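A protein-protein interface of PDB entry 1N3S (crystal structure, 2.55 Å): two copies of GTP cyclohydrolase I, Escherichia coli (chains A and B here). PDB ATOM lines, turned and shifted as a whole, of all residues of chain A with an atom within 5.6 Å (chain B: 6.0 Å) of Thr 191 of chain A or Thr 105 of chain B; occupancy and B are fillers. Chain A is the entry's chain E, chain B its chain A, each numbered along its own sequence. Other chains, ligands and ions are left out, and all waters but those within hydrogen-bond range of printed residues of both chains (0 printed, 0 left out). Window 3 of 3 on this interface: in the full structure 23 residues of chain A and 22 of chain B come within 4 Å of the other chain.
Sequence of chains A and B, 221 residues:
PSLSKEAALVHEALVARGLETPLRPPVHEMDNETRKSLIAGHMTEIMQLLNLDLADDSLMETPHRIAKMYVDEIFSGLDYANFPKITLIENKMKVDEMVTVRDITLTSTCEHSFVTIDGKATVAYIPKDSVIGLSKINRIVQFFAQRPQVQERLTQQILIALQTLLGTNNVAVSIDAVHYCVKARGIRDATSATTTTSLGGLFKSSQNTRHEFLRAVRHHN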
ATOM      1  N   ARG A 188      -1.958  -4.278  18.815  1.00  0.00           N
ATOM      2  CA  ARG A 188      -2.204  -4.445  17.378  1.00  0.00           C
ATOM      3  C   ARG A 188      -0.954  -4.315  16.487  1.00  0.00           C
ATOM      4  O   ARG A 188      -0.897  -3.477  15.572  1.00  0.00           O
ATOM      5  CB  ARG A 188      -3.348  -3.516  16.929  1.00  0.00           C
ATOM      6  CG  ARG A 188      -4.713  -3.990  17.396  1.00  0.00           C
ATOM      7  CD  ARG A 188      -5.808  -2.951  17.199  1.00  0.00           C
ATOM      8  NE  ARG A 188      -7.041  -3.550  16.678  1.00  0.00           N
ATOM      9  CZ  ARG A 188      -7.877  -4.333  17.363  1.00  0.00           C
ATOM     10  NH1 ARG A 188      -7.639  -4.640  18.631  1.00  0.00           N
ATOM     11  NH2 ARG A 188      -8.953  -4.831  16.762  1.00  0.00           N
ATOM     12  N   ASP A 189       0.061  -5.118  16.827  1.00  0.00           N
ATOM     13  CA  ASP A 189       1.345  -5.147  16.119  1.00  0.00           C
ATOM     14  C   ASP A 189       1.294  -6.180  14.989  1.00  0.00           C
ATOM     15  O   ASP A 189       1.570  -7.377  15.196  1.00  0.00           O
ATOM     16  CB  ASP A 189       2.490  -5.464  17.099  1.00  0.00           C
ATOM     17  CG  ASP A 189       3.823  -4.856  16.668  1.00  0.00           C
ATOM     18  OD1 ASP A 189       4.239  -5.033  15.495  1.00  0.00           O
ATOM     19  OD2 ASP A 189       4.467  -4.198  17.514  1.00  0.00           O
ATOM     20  N   ALA A 190       0.974  -5.683  13.792  1.00  0.00           N
ATOM     21  CA  ALA A 190       0.831  -6.510  12.594  1.00  0.00           C
ATOM     22  C   ALA A 190       2.104  -7.141  12.035  1.00  0.00           C
ATOM     23  O   ALA A 190       2.041  -8.186  11.376  1.00  0.00           O
ATOM     24  CB  ALA A 190       0.109  -5.729  11.510  1.00  0.00           C
ATOM     25  N   THR A 191       3.254  -6.549  12.355  1.00  0.00           N
ATOM     26  CA  THR A 191       4.533  -7.042  11.850  1.00  0.00           C
ATOM     27  C   THR A 191       5.419  -7.862  12.801  1.00  0.00           C
ATOM     28  O   THR A 191       6.175  -8.724  12.335  1.00  0.00           O
ATOM     29  CB  THR A 191       5.372  -5.894  11.212  1.00  0.00           C
ATOM     30  OG1 THR A 191       5.791  -4.960  12.215  1.00  0.00           O
ATOM     31  CG2 THR A 191       4.565  -5.139  10.141  1.00  0.00           C
ATOM     32  N   SER A 192       5.327  -7.624  14.113  1.00  0.00           N
ATOM     33  CA  SER A 192       6.150  -8.359  15.093  1.00  0.00           C
ATOM     34  C   SER A 192       5.946  -9.866  15.242  1.00  0.00           C
ATOM     35  O   SER A 192       4.848 -10.397  15.057  1.00  0.00           O
ATOM     36  CB  SER A 192       6.101  -7.696  16.491  1.00  0.00           C
ATOM     37  OG  SER A 192       5.043  -8.192  17.316  1.00  0.00           O
ATOM     38  N   ALA A 193       7.035 -10.523  15.626  1.00  0.00           N
ATOM     39  CA  ALA A 193       7.078 -11.957  15.876  1.00  0.00           C
ATOM     40  C   ALA A 193       8.074 -12.147  17.008  1.00  0.00           C
ATOM     41  O   ALA A 193       8.981 -11.322  17.200  1.00  0.00           O
ATOM     42  CB  ALA A 193       7.544 -12.709  14.635  1.00  0.00           C
ATOM     43  N   ARG B 102      11.357  -9.330  17.344  1.00  0.00           N
ATOM     44  CA  ARG B 102      11.780  -8.516  16.205  1.00  0.00           C
ATOM     45  C   ARG B 102      10.599  -7.923  15.466  1.00  0.00           C
ATOM     46  O   ARG B 102       9.452  -8.311  15.704  1.00  0.00           O
ATOM     47  CB  ARG B 102      12.652  -9.335  15.230  1.00  0.00           C
ATOM     48  CG  ARG B 102      11.909 -10.348  14.351  1.00  0.00           C
ATOM     49  CD  ARG B 102      11.866 -11.757  14.954  1.00  0.00           C
ATOM     50  NE  ARG B 102      11.009 -12.714  14.234  1.00  0.00           N
ATOM     51  CZ  ARG B 102      11.009 -12.945  12.918  1.00  0.00           C
ATOM     52  NH1 ARG B 102      11.824 -12.293  12.099  1.00  0.00           N
ATOM     53  NH2 ARG B 102      10.171 -13.846  12.418  1.00  0.00           N
ATOM     54  N   ASP B 103      10.920  -7.032  14.525  1.00  0.00           N
ATOM     55  CA  ASP B 103       9.966  -6.339  13.665  1.00  0.00           C
ATOM     56  C   ASP B 103       8.823  -5.629  14.385  1.00  0.00           C
ATOM     57  O   ASP B 103       7.675  -5.652  13.926  1.00  0.00           O
ATOM     58  CB  ASP B 103       9.443  -7.282  12.557  1.00  0.00           C
ATOM     59  CG  ASP B 103      10.468  -7.522  11.446  1.00  0.00           C
ATOM     60  OD1 ASP B 103      11.168  -6.560  11.027  1.00  0.00           O
ATOM     61  OD2 ASP B 103      10.559  -8.678  10.978  1.00  0.00           O
ATOM     62  N   ILE B 104       9.159  -4.974  15.498  1.00  0.00           N
ATOM     63  CA  ILE B 104       8.186  -4.238  16.314  1.00  0.00           C
ATOM     64  C   ILE B 104       7.835  -2.952  15.594  1.00  0.00           C
ATOM     65  O   ILE B 104       8.730  -2.196  15.231  1.00  0.00           O
ATOM     66  CB  ILE B 104       8.739  -3.897  17.743  1.00  0.00           C
ATOM     67  CG1 ILE B 104       9.042  -5.190  18.512  1.00  0.00           C
ATOM     68  CG2 ILE B 104       7.742  -3.032  18.522  1.00  0.00           C
ATOM     69  CD1 ILE B 104       9.987  -5.020  19.697  1.00  0.00           C
ATOM     70  N   THR B 105       6.537  -2.720  15.387  1.00  0.00           N
ATOM     71  CA  THR B 105       6.047  -1.510  14.720  1.00  0.00           C
ATOM     72  C   THR B 105       6.398  -0.307  15.599  1.00  0.00           C
ATOM     73  O   THR B 105       6.053  -0.272  16.782  1.00  0.00           O
ATOM     74  CB  THR B 105       4.509  -1.583  14.488  1.00  0.00           C
ATOM     75  OG1 THR B 105       4.195  -2.758  13.732  1.00  0.00           O
ATOM     76  CG2 THR B 105       3.996  -0.369  13.733  1.00  0.00           C
ATOM     77  N   LEU B 106       7.206   0.589  15.045  1.00  0.00           N
ATOM     78  CA  LEU B 106       7.634   1.784  15.747  1.00  0.00           C
ATOM     79  C   LEU B 106       7.259   3.008  14.925  1.00  0.00           C
ATOM     80  O   LEU B 106       7.699   3.176  13.780  1.00  0.00           O
ATOM     81  CB  LEU B 106       9.145   1.735  16.035  1.00  0.00           C
ATOM     82  CG  LEU B 106       9.885   2.865  16.765  1.00  0.00           C
ATOM     83  CD1 LEU B 106      11.012   2.275  17.570  1.00  0.00           C
ATOM     84  CD2 LEU B 106      10.434   3.943  15.817  1.00  0.00           C
ATOM     85  N   THR B 107       6.416   3.844  15.527  1.00  0.00           N
ATOM     86  CA  THR B 107       5.943   5.080  14.915  1.00  0.00           C
ATOM     87  C   THR B 107       6.402   6.244  15.780  1.00  0.00           C
ATOM     88  O   THR B 107       6.027   6.352  16.948  1.00  0.00           O
ATOM     89  CB  THR B 107       4.407   5.081  14.765  1.00  0.00           C
ATOM     90  OG1 THR B 107       3.791   4.865  16.039  1.00  0.00           O
ATOM     91  CG2 THR B 107       3.972   3.972  13.788  1.00  0.00           C
ATOM     92  N   GLY B 119       9.674   3.204  11.533  1.00  0.00           N
ATOM     93  CA  GLY B 119      10.684   2.292  12.015  1.00  0.00           C
ATOM     94  C   GLY B 119      10.255   0.920  12.475  1.00  0.00           C
ATOM     95  O   GLY B 119       9.060   0.591  12.538  1.00  0.00           O
ATOM     96  N   LYS B 120      11.272   0.103  12.735  1.00  0.00           N
ATOM     97  CA  LYS B 120      11.131  -1.260  13.213  1.00  0.00           C
ATOM     98  C   LYS B 120      12.144  -1.482  14.325  1.00  0.00           C
ATOM     99  O   LYS B 120      13.319  -1.124  14.197  1.00  0.00           O
ATOM    100  CB  LYS B 120      11.357  -2.282  12.089  1.00  0.00           C
ATOM    101  CG  LYS B 120      10.071  -2.897  11.553  1.00  0.00           C
ATOM    102  CD  LYS B 120       9.415  -2.058  10.451  1.00  0.00           C
ATOM    103  CE  LYS B 120       7.917  -2.301  10.398  1.00  0.00           C
ATOM    104  NZ  LYS B 120       7.614  -3.756  10.330  1.00  0.00           N
ATOM    105  N   ALA B 121      11.672  -2.058  15.421  1.00  0.00           N
ATOM    106  CA  ALA B 121      12.527  -2.323  16.561  1.00  0.00           C
ATOM    107  C   ALA B 121      12.751  -3.795  16.822  1.00  0.00           C
ATOM    108  O   ALA B 121      11.874  -4.636  16.608  1.00  0.00           O
ATOM    109  CB  ALA B 121      11.977  -1.641  17.808  1.00  0.00           C
ATOM    110  N   ASN B 138       6.523  -4.473  23.125  1.00  0.00           N
ATOM    111  CA  ASN B 138       5.973  -3.719  21.982  1.00  0.00           C
ATOM    112  C   ASN B 138       5.421  -2.375  22.461  1.00  0.00           C
ATOM    113  O   ASN B 138       5.656  -1.350  21.825  1.00  0.00           O
ATOM    114  CB  ASN B 138       4.817  -4.475  21.298  1.00  0.00           C
ATOM    115  CG  ASN B 138       5.204  -5.861  20.794  1.00  0.00           C
ATOM    116  OD1 ASN B 138       5.185  -6.117  19.594  1.00  0.00           O
ATOM    117  ND2 ASN B 138       5.464  -6.780  21.709  1.00  0.00           N
ATOM    118  N   VAL B 141       8.223   0.115  23.669  1.00  0.00           N
ATOM    119  CA  VAL B 141       8.848   0.642  22.459  1.00  0.00           C
ATOM    120  C   VAL B 141       8.026   1.800  21.925  1.00  0.00           C
ATOM    121  O   VAL B 141       8.554   2.902  21.751  1.00  0.00           O
ATOM    122  CB  VAL B 141       9.023  -0.466  21.383  1.00  0.00           C
ATOM    123  CG1 VAL B 141       9.513   0.126  20.077  1.00  0.00           C
ATOM    124  CG2 VAL B 141      10.026  -1.502  21.860  1.00  0.00           C
ATOM    125  N   GLN B 142       6.718   1.563  21.801  1.00  0.00           N
ATOM    126  CA  GLN B 142       5.778   2.563  21.311  1.00  0.00           C
ATOM    127  C   GLN B 142       5.559   3.767  22.219  1.00  0.00           C
ATOM    128  O   GLN B 142       5.438   4.879  21.716  1.00  0.00           O
ATOM    129  CB  GLN B 142       4.456   1.922  20.882  1.00  0.00           C
ATOM    130  CG  GLN B 142       4.505   1.336  19.453  1.00  0.00           C
ATOM    131  CD  GLN B 142       4.530   2.403  18.346  1.00  0.00           C
ATOM    132  OE1 GLN B 142       5.509   3.133  18.174  1.00  0.00           O
ATOM    133  NE2 GLN B 142       3.451   2.475  17.583  1.00  0.00           N
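The guanidinium group of Arg 102 of chain B is in salt-bridge range of the side-chain carboxylate of Asp 103 of chain B.
The backbone NH (N) of Asp 103 of chain B sits at hydrogen-bond distance from the backbone carbonyl oxygen (O) of Ala 121 of chain B (3.3 Å).
The backbone carbonyl oxygen (O) of Ile 104 of chain B is in hydrogen-bond range of the backbone NH (N) of Ala 121 of chain B.
OD1 of Asp 189 of chain A is in hydrogen-bond range of N of Ser 192 of chain A.
Hydrophobic or aromatic side chains of chain A within 4 Å of the printed part of chain B: Ala 193.
Hydrophobic or aromatic side chains of chain B that line the printed part of chain A: Ile 104.
Among the printed residues, 11 pairs touch across the chains.
The backbone NH of Arg 102 of chain B sits at hydrogen-bond distance from the backbone carbonyl oxygen of Ala 193 of chain A.
The backbone carbonyl oxygen (O) of Asp 103 of chain B sits at hydrogen-bond distance from the side-chain hydroxyl (OG1) of Thr 191 of chain A, 2.6 Å away.
The backbone carbonyl oxygen (O) of Asp 103 of chain B sits at hydrogen-bond distance from the backbone NH (N) of Ser 192 of chain A (3.1 Å).
The side-chain hydroxyl (OG1) of Thr 105 of chain B is in hydrogen-bond range of the side-chain carboxylate (OD1) of Asp 189 of chain A, at 2.9 Å.
The side-chain hydroxyl (OG1) of Thr 105 of chain B lies within hydrogen-bond range of the side-chain hydroxyl (OG1) of Thr 191 of chain A, at 3.1 Å.
The side-chain amino group of Lys 120 of chain B lies within hydrogen-bond range of the side-chain hydroxyl of Thr 191 of chain A, 2.9 Å away.
The side-chain amide oxygen of Asn 138 of chain B sits close to the side-chain carboxylate of Asp 189 of chain A (2.9 Å).
The side-chain hydroxyl of Ser 192 of chain A sits at hydrogen-bond distance from the side-chain amide oxygen of Asn 138 of chain B (3.1 Å).
Among the printed residues, merely in contact across the chains: Asp 189 of chain A with Asp 103 of chain B (3.8 Å), Asp 189 of chain A with Ile 104 of chain B (3.6 Å) and Ser 192 of chain A with Arg 102 of chain B (3.4 Å).
No position is printed for both chains.
Printed residues of chain B within 4 Å of Asp 189 of chain A: Asp 103, Ile 104, Thr 105 and Asn 138.
Of chain B, only Asp 103 (2.6 Å), Thr 105 (3.1 Å) and Lys 120 (2.9 Å) come within 4 Å of Thr 191 of chain A.
Of the printed residues of chain B, Ala 193 of chain A touches Arg 102.
Of chain A, only Asp 189 (2.9 Å) and Thr 191 (3.1 Å) come within 4 Å of Thr 105 of chain B.
Gly 119 of chain B touches none of the printed residues of chain A.
Ala 121 of chain B touches none of the printed residues of chain A.
The nearest residue of chain B that does not touch Thr 191 of chain A is Ile 104 of chain B (4.4 Å).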
